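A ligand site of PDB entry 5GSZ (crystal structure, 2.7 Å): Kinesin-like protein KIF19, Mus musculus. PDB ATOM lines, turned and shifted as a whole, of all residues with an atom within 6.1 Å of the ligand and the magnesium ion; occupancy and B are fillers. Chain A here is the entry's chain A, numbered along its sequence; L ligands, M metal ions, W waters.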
ATOM      1  N   ARG A  17       3.262  29.876  11.666  1.00  0.00           N
ATOM      2  CA  ARG A  17       3.463  29.434  13.037  1.00  0.00           C
ATOM      3  C   ARG A  17       4.865  29.801  13.512  1.00  0.00           C
ATOM      4  O   ARG A  17       5.851  29.399  12.893  1.00  0.00           O
ATOM      5  CB  ARG A  17       3.260  27.938  13.181  1.00  0.00           C
ATOM      6  CG  ARG A  17       3.207  27.470  14.625  1.00  0.00           C
ATOM      7  CD  ARG A  17       2.744  26.051  14.666  1.00  0.00           C
ATOM      8  NE  ARG A  17       2.455  25.599  15.997  1.00  0.00           N
ATOM      9  CZ  ARG A  17       2.016  24.386  16.287  1.00  0.00           C
ATOM     10  NH1 ARG A  17       1.830  23.521  15.302  1.00  0.00           N
ATOM     11  NH2 ARG A  17       1.769  24.037  17.533  1.00  0.00           N
ATOM     12  N   VAL A  18       4.933  30.517  14.625  1.00  0.00           N
ATOM     13  CA  VAL A  18       6.189  30.803  15.318  1.00  0.00           C
ATOM     14  C   VAL A  18       6.343  29.804  16.461  1.00  0.00           C
ATOM     15  O   VAL A  18       5.505  29.745  17.365  1.00  0.00           O
ATOM     16  CB  VAL A  18       6.211  32.244  15.852  1.00  0.00           C
ATOM     17  CG1 VAL A  18       7.622  32.605  16.268  1.00  0.00           C
ATOM     18  CG2 VAL A  18       5.635  33.218  14.813  1.00  0.00           C
ATOM     19  N   ARG A  19       7.397  29.019  16.421  1.00  0.00           N
ATOM     20  CA  ARG A  19       7.610  28.131  17.553  1.00  0.00           C
ATOM     21  C   ARG A  19       8.252  28.926  18.683  1.00  0.00           C
ATOM     22  O   ARG A  19       8.839  29.975  18.445  1.00  0.00           O
ATOM     23  CB  ARG A  19       8.479  26.956  17.164  1.00  0.00           C
ATOM     24  CG  ARG A  19       9.854  27.338  16.696  1.00  0.00           C
ATOM     25  CD  ARG A  19      10.719  26.101  16.586  1.00  0.00           C
ATOM     26  NE  ARG A  19      12.089  26.378  16.169  1.00  0.00           N
ATOM     27  CZ  ARG A  19      12.990  27.007  16.921  1.00  0.00           C
ATOM     28  NH1 ARG A  19      12.656  27.476  18.122  1.00  0.00           N
ATOM     29  NH2 ARG A  19      14.234  27.199  16.480  1.00  0.00           N
ATOM     30  N   PRO A  20       8.131  28.476  19.920  1.00  0.00           N
ATOM     31  CA  PRO A  20       8.886  29.127  21.002  1.00  0.00           C
ATOM     32  C   PRO A  20      10.384  29.097  20.717  1.00  0.00           C
ATOM     33  O   PRO A  20      10.888  28.200  20.035  1.00  0.00           O
ATOM     34  CB  PRO A  20       8.544  28.292  22.229  1.00  0.00           C
ATOM     35  CG  PRO A  20       7.254  27.607  21.875  1.00  0.00           C
ATOM     36  CD  PRO A  20       7.301  27.369  20.409  1.00  0.00           C
ATOM     37  N   PHE A  73       3.643  30.709  20.482  1.00  0.00           N
ATOM     38  CA  PHE A  73       3.642  29.734  21.576  1.00  0.00           C
ATOM     39  C   PHE A  73       2.329  29.685  22.348  1.00  0.00           C
ATOM     40  O   PHE A  73       2.092  28.731  23.085  1.00  0.00           O
ATOM     41  CB  PHE A  73       4.776  30.029  22.574  1.00  0.00           C
ATOM     42  CG  PHE A  73       4.607  31.337  23.303  1.00  0.00           C
ATOM     43  CD1 PHE A  73       4.776  32.547  22.621  1.00  0.00           C
ATOM     44  CD2 PHE A  73       4.262  31.368  24.648  1.00  0.00           C
ATOM     45  CE1 PHE A  73       4.622  33.747  23.281  1.00  0.00           C
ATOM     46  CE2 PHE A  73       4.117  32.568  25.310  1.00  0.00           C
ATOM     47  CZ  PHE A  73       4.298  33.768  24.621  1.00  0.00           C
ATOM     48  N   GLN A  77      -1.841  22.732  20.090  1.00  0.00           N
ATOM     49  CA  GLN A  77      -1.989  21.869  18.927  1.00  0.00           C
ATOM     50  C   GLN A  77      -3.423  21.899  18.397  1.00  0.00           C
ATOM     51  O   GLN A  77      -3.636  22.127  17.198  1.00  0.00           O
ATOM     52  CB  GLN A  77      -1.527  20.452  19.267  1.00  0.00           C
ATOM     53  CG  GLN A  77      -0.007  20.340  19.473  1.00  0.00           C
ATOM     54  CD  GLN A  77       0.816  20.302  18.189  1.00  0.00           C
ATOM     55  OE1 GLN A  77       0.871  21.282  17.440  1.00  0.00           O
ATOM     56  NE2 GLN A  77       1.497  19.180  17.946  1.00  0.00           N
ATOM     57  N   GLY A 104       8.911  25.121   5.884  1.00  0.00           N
ATOM     58  CA  GLY A 104       9.817  25.952   6.637  1.00  0.00           C
ATOM     59  C   GLY A 104      11.168  25.301   6.797  1.00  0.00           C
ATOM     60  O   GLY A 104      11.368  24.135   6.467  1.00  0.00           O
ATOM     61  N   PRO A 105      12.125  26.069   7.310  1.00  0.00           N
ATOM     62  CA  PRO A 105      13.479  25.531   7.500  1.00  0.00           C
ATOM     63  C   PRO A 105      13.492  24.465   8.585  1.00  0.00           C
ATOM     64  O   PRO A 105      12.612  24.400   9.442  1.00  0.00           O
ATOM     65  CB  PRO A 105      14.284  26.761   7.932  1.00  0.00           C
ATOM     66  CG  PRO A 105      13.410  27.931   7.679  1.00  0.00           C
ATOM     67  CD  PRO A 105      12.002  27.459   7.753  1.00  0.00           C
ATOM     68  N   THR A 106      14.518  23.608   8.537  1.00  0.00           N
ATOM     69  CA  THR A 106      14.668  22.554   9.533  1.00  0.00           C
ATOM     70  C   THR A 106      14.679  23.110  10.957  1.00  0.00           C
ATOM     71  O   THR A 106      15.283  24.150  11.231  1.00  0.00           O
ATOM     72  CB  THR A 106      15.961  21.780   9.267  1.00  0.00           C
ATOM     73  OG1 THR A 106      15.909  21.186   7.971  1.00  0.00           O
ATOM     74  CG2 THR A 106      16.166  20.701  10.304  1.00  0.00           C
ATOM     75  N   GLY A 107      13.993  22.419  11.857  1.00  0.00           N
ATOM     76  CA  GLY A 107      13.993  22.791  13.257  1.00  0.00           C
ATOM     77  C   GLY A 107      12.982  23.835  13.666  1.00  0.00           C
ATOM     78  O   GLY A 107      12.936  24.186  14.867  1.00  0.00           O
ATOM     79  N   CYS A 108      12.153  24.322  12.714  1.00  0.00           N
ATOM     80  CA  CYS A 108      11.160  25.379  12.952  1.00  0.00           C
ATOM     81  C   CYS A 108       9.770  24.873  13.287  1.00  0.00           C
ATOM     82  O   CYS A 108       8.894  25.688  13.599  1.00  0.00           O
ATOM     83  CB  CYS A 108      11.014  26.288  11.717  1.00  0.00           C
ATOM     84  SG  CYS A 108      12.402  27.308  11.300  1.00  0.00           S
ATOM     85  N   GLY A 109       9.503  23.571  13.167  1.00  0.00           N
ATOM     86  CA  GLY A 109       8.216  23.078  13.620  1.00  0.00           C
ATOM     87  C   GLY A 109       7.433  22.117  12.758  1.00  0.00           C
ATOM     88  O   GLY A 109       6.435  21.571  13.245  1.00  0.00           O
ATOM     89  N   LYS A 110       7.859  21.847  11.521  1.00  0.00           N
ATOM     90  CA  LYS A 110       7.054  21.088  10.574  1.00  0.00           C
ATOM     91  C   LYS A 110       6.559  19.754  11.162  1.00  0.00           C
ATOM     92  O   LYS A 110       5.350  19.530  11.276  1.00  0.00           O
ATOM     93  CB  LYS A 110       7.852  20.868   9.284  1.00  0.00           C
ATOM     94  CG  LYS A 110       8.112  22.172   8.526  1.00  0.00           C
ATOM     95  CD  LYS A 110       8.788  21.924   7.187  1.00  0.00           C
ATOM     96  CE  LYS A 110      10.046  21.080   7.330  1.00  0.00           C
ATOM     97  NZ  LYS A 110      11.126  21.681   8.176  1.00  0.00           N
ATOM     98  N   THR A 111       7.478  18.858  11.528  1.00  0.00           N
ATOM     99  CA  THR A 111       7.034  17.558  12.050  1.00  0.00           C
ATOM    100  C   THR A 111       6.198  17.727  13.329  1.00  0.00           C
ATOM    101  O   THR A 111       5.270  16.954  13.555  1.00  0.00           O
ATOM    102  CB  THR A 111       8.237  16.652  12.291  1.00  0.00           C
ATOM    103  OG1 THR A 111       9.025  16.562  11.098  1.00  0.00           O
ATOM    104  CG2 THR A 111       7.792  15.256  12.650  1.00  0.00           C
ATOM    105  N   TYR A 112       6.480  18.737  14.143  1.00  0.00           N
ATOM    106  CA  TYR A 112       5.669  18.967  15.329  1.00  0.00           C
ATOM    107  C   TYR A 112       4.229  19.344  14.957  1.00  0.00           C
ATOM    108  O   TYR A 112       3.273  18.819  15.551  1.00  0.00           O
ATOM    109  CB  TYR A 112       6.300  20.040  16.226  1.00  0.00           C
ATOM    110  CG  TYR A 112       5.514  20.339  17.490  1.00  0.00           C
ATOM    111  CD1 TYR A 112       5.691  19.572  18.635  1.00  0.00           C
ATOM    112  CD2 TYR A 112       4.566  21.366  17.524  1.00  0.00           C
ATOM    113  CE1 TYR A 112       4.983  19.842  19.803  1.00  0.00           C
ATOM    114  CE2 TYR A 112       3.849  21.635  18.681  1.00  0.00           C
ATOM    115  CZ  TYR A 112       4.059  20.857  19.812  1.00  0.00           C
ATOM    116  OH  TYR A 112       3.354  21.115  20.962  1.00  0.00           O
ATOM    117  N   THR A 113       4.058  20.260  13.992  1.00  0.00           N
ATOM    118  CA  THR A 113       2.721  20.641  13.546  1.00  0.00           C
ATOM    119  C   THR A 113       1.961  19.456  12.954  1.00  0.00           C
ATOM    120  O   THR A 113       0.773  19.300  13.238  1.00  0.00           O
ATOM    121  CB  THR A 113       2.798  21.775  12.519  1.00  0.00           C
ATOM    122  OG1 THR A 113       3.027  23.020  13.179  1.00  0.00           O
ATOM    123  CG2 THR A 113       1.489  21.878  11.708  1.00  0.00           C
ATOM    124  N   THR A 117       3.520  14.947  19.082  1.00  0.00           N
ATOM    125  CA  THR A 117       4.086  13.970  19.997  1.00  0.00           C
ATOM    126  C   THR A 117       2.963  13.190  20.670  1.00  0.00           C
ATOM    127  O   THR A 117       1.790  13.569  20.587  1.00  0.00           O
ATOM    128  CB  THR A 117       4.953  14.623  21.078  1.00  0.00           C
ATOM    129  OG1 THR A 117       4.124  15.469  21.894  1.00  0.00           O
ATOM    130  CG2 THR A 117       6.055  15.439  20.469  1.00  0.00           C
ATOM    131  N   ARG A 206      11.985   7.079   7.806  1.00  0.00           N
ATOM    132  CA  ARG A 206      12.475   8.143   6.927  1.00  0.00           C
ATOM    133  C   ARG A 206      13.998   8.115   6.861  1.00  0.00           C
ATOM    134  O   ARG A 206      14.684   7.985   7.886  1.00  0.00           O
ATOM    135  CB  ARG A 206      12.006   9.505   7.437  1.00  0.00           C
ATOM    136  CG  ARG A 206      10.502   9.663   7.494  1.00  0.00           C
ATOM    137  CD  ARG A 206      10.078  11.006   8.105  1.00  0.00           C
ATOM    138  NE  ARG A 206      10.167  12.187   7.239  1.00  0.00           N
ATOM    139  CZ  ARG A 206       9.705  13.385   7.614  1.00  0.00           C
ATOM    140  NH1 ARG A 206       9.138  13.508   8.810  1.00  0.00           N
ATOM    141  NH2 ARG A 206       9.766  14.451   6.816  1.00  0.00           N
ATOM    142  N   THR A 216      16.562  12.511  11.179  1.00  0.00           N
ATOM    143  CA  THR A 216      15.875  12.473   9.885  1.00  0.00           C
ATOM    144  C   THR A 216      16.481  13.500   8.928  1.00  0.00           C
ATOM    145  O   THR A 216      16.680  14.655   9.296  1.00  0.00           O
ATOM    146  CB  THR A 216      14.380  12.752  10.044  1.00  0.00           C
ATOM    147  OG1 THR A 216      13.738  11.679  10.745  1.00  0.00           O
ATOM    148  CG2 THR A 216      13.699  12.958   8.676  1.00  0.00           C
ATOM    149  N   SER A 217      16.739  13.076   7.689  1.00  0.00           N
ATOM    150  CA  SER A 217      17.291  13.989   6.704  1.00  0.00           C
ATOM    151  C   SER A 217      16.393  15.206   6.524  1.00  0.00           C
ATOM    152  O   SER A 217      15.157  15.112   6.539  1.00  0.00           O
ATOM    153  CB  SER A 217      17.482  13.294   5.368  1.00  0.00           C
ATOM    154  OG  SER A 217      17.753  14.261   4.360  1.00  0.00           O
ATOM    155  N   ASP A 250       4.511  16.673   5.273  1.00  0.00           N
ATOM    156  CA  ASP A 250       5.638  17.206   6.032  1.00  0.00           C
ATOM    157  C   ASP A 250       6.798  17.373   5.059  1.00  0.00           C
ATOM    158  O   ASP A 250       7.499  16.414   4.732  1.00  0.00           O
ATOM    159  CB  ASP A 250       5.997  16.238   7.156  1.00  0.00           C
ATOM    160  CG  ASP A 250       7.050  16.799   8.103  1.00  0.00           C
ATOM    161  OD1 ASP A 250       7.287  18.029   8.113  1.00  0.00           O
ATOM    162  OD2 ASP A 250       7.659  15.997   8.855  1.00  0.00           O
ATOM    163  N   LEU A 251       7.013  18.605   4.587  1.00  0.00           N
ATOM    164  CA  LEU A 251       7.939  18.837   3.487  1.00  0.00           C
ATOM    165  C   LEU A 251       9.393  18.668   3.922  1.00  0.00           C
ATOM    166  O   LEU A 251       9.728  18.559   5.100  1.00  0.00           O
ATOM    167  CB  LEU A 251       7.780  20.245   2.914  1.00  0.00           C
ATOM    168  CG  LEU A 251       6.540  20.558   2.083  1.00  0.00           C
ATOM    169  CD1 LEU A 251       6.515  22.004   1.671  1.00  0.00           C
ATOM    170  CD2 LEU A 251       6.541  19.664   0.887  1.00  0.00           C
ATOM    171  N   HIS A 322       6.498  27.828   8.898  1.00  0.00           N
ATOM    172  CA  HIS A 322       7.079  27.769  10.235  1.00  0.00           C
ATOM    173  C   HIS A 322       8.350  28.597  10.316  1.00  0.00           C
ATOM    174  O   HIS A 322       9.182  28.525   9.404  1.00  0.00           O
ATOM    175  CB  HIS A 322       7.393  26.313  10.615  1.00  0.00           C
ATOM    176  CG  HIS A 322       6.184  25.429  10.661  1.00  0.00           C
ATOM    177  ND1 HIS A 322       5.638  24.865   9.525  1.00  0.00           N
ATOM    178  CD2 HIS A 322       5.416  25.031  11.692  1.00  0.00           C
ATOM    179  CE1 HIS A 322       4.578  24.153   9.865  1.00  0.00           C
ATOM    180  NE2 HIS A 322       4.418  24.243  11.184  1.00  0.00           N
HETATM  181  P1  LIG L   1      11.106  20.385  11.581  1.00  0.00           P
HETATM  182  O1  LIG L   1      10.129  19.229  11.500  1.00  0.00           O
HETATM  183  O2  LIG L   1      10.601  21.578  10.808  1.00  0.00           O
HETATM  184  O3  LIG L   1      12.541  20.000  11.372  1.00  0.00           O
HETATM  185  P2  LIG L   1      10.653  19.809  14.292  1.00  0.00           P
HETATM  186  O4  LIG L   1       9.226  20.079  14.657  1.00  0.00           O
HETATM  187  O5  LIG L   1      11.119  18.434  13.865  1.00  0.00           O
HETATM  188  O6  LIG L   1      11.108  20.853  13.135  1.00  0.00           O
HETATM  189  O7  LIG L   1      11.627  20.135  15.515  1.00  0.00           O
HETATM  190  C1  LIG L   1      11.482  21.255  16.378  1.00  0.00           C
HETATM  191  C2  LIG L   1      11.750  20.767  17.786  1.00  0.00           C
HETATM  192  O8  LIG L   1      11.093  21.671  18.656  1.00  0.00           O
HETATM  193  C3  LIG L   1      11.057  19.441  17.973  1.00  0.00           C
HETATM  194  O9  LIG L   1      11.713  18.807  19.084  1.00  0.00           O
HETATM  195  C4  LIG L   1       9.641  19.820  18.319  1.00  0.00           C
HETATM  196  O10 LIG L   1       9.070  18.880  19.232  1.00  0.00           O
HETATM  197  C5  LIG L   1       9.793  21.186  18.994  1.00  0.00           C
HETATM  198  N1  LIG L   1       8.780  22.161  18.513  1.00  0.00           N
HETATM  199  C6  LIG L   1       8.613  22.593  17.240  1.00  0.00           C
HETATM  200  N2  LIG L   1       7.609  23.496  17.145  1.00  0.00           N
HETATM  201  C7  LIG L   1       7.106  23.655  18.379  1.00  0.00           C
HETATM  202  C8  LIG L   1       6.021  24.445  18.974  1.00  0.00           C
HETATM  203  N3  LIG L   1       5.273  25.273  18.206  1.00  0.00           N
HETATM  204  N4  LIG L   1       5.816  24.304  20.298  1.00  0.00           N
HETATM  205  C9  LIG L   1       6.574  23.497  21.066  1.00  0.00           C
HETATM  206  N5  LIG L   1       7.568  22.737  20.585  1.00  0.00           N
HETATM  207  C10 LIG L   1       7.875  22.770  19.279  1.00  0.00           C
HETATM  208 MG    MG M   1      10.908  17.221  10.332  1.00  0.00          MG
HETATM  209  O   HOH W   1      12.999  18.276  10.071  1.00  0.00           O
HETATM  210  O   HOH W   2       9.988  18.167   8.555  1.00  0.00           O
HETATM  211  O   HOH W   3      11.317  15.204  10.111  1.00  0.00           O
HETATM  212  O   HOH W   4      11.595  16.936  12.106  1.00  0.00           O
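Water W2 bridges OD1 of Asp 250 and O of Leu 251.
NE of Arg 17 touches N3 of the ligand (3.6 Å).
Arg 19 touches the ligand.
CD of Pro 20 touches N4 of the ligand (3.4 Å).
Pro 105 touches the ligand (O to O2, 3.7 Å).
Thr 106 touches the ligand.
N of Cys 108 touches O6 of the ligand (3.6 Å).
Hydrophobic or aromatic side chains that line the ligand: Pro 20 and Tyr 112.
Of the 23 residues printed, 11 come within 4 Å of the ligand.
The magnesium ion is bound by water W4 (1.9 Å), water W3 (2.1 Å), the side-chain hydroxyl (OG1) of Thr 111 (2.1 Å), water W2 (2.2 Å), water W1 (2.4 Å) and an oxygen (O1) of the ligand (2.5 Å).
Residues that only touch the magnesium ion: Asp 250 (3.8 Å).
Along chain A the residues within 4 Å of the magnesium ion span positions 111 to 250.
The side-chain amide oxygen (OE1) of Gln 77 lies within hydrogen-bond range of the guanidinium group (NH2) of Arg 17 (2.9 Å).
OD2 of Asp 250 is in salt-bridge range of NH1 of Arg 206 (2.9 Å).
O of Tyr 112 lies within hydrogen-bond range of NE2 of Gln 77 (3.0 Å).
The side-chain sulfur (SG) of Cys 108 sits close to the backbone carbonyl oxygen (O) of Pro 105, 3.5 Å away.
The side-chain carboxylate (OD2) of Asp 250 lies close to the side-chain hydroxyl (OG1) of Thr 111 (2.7 Å).
O of Gly 107 sits at hydrogen-bond distance from NE of Arg 19, at 2.7 Å.
The side-chain amino group (NZ) of Lys 110 is in hydrogen-bond range of the backbone carbonyl oxygen (O) of Gly 104, 3.0 Å away.
O of Pro 105 sits at hydrogen-bond distance from NZ of Lys 110.
O2 of the ligand lies within hydrogen-bond range of N of Lys 110 (2.8 Å).
The backbone NH (N) of Tyr 112 sits at hydrogen-bond distance from an oxygen (O4) of the ligand (3.1 Å).
O3 of the ligand lies within hydrogen-bond range of N of Gly 107, at 2.9 Å.
N of Gly 109 is in hydrogen-bond range of O6 of the ligand (3.2 Å).
An oxygen (O1) of the ligand lies close to the backbone NH of Thr 111, 2.7 Å away.
NZ of Lys 110 lies within salt-bridge range of O2 of the ligand (2.7 Å).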
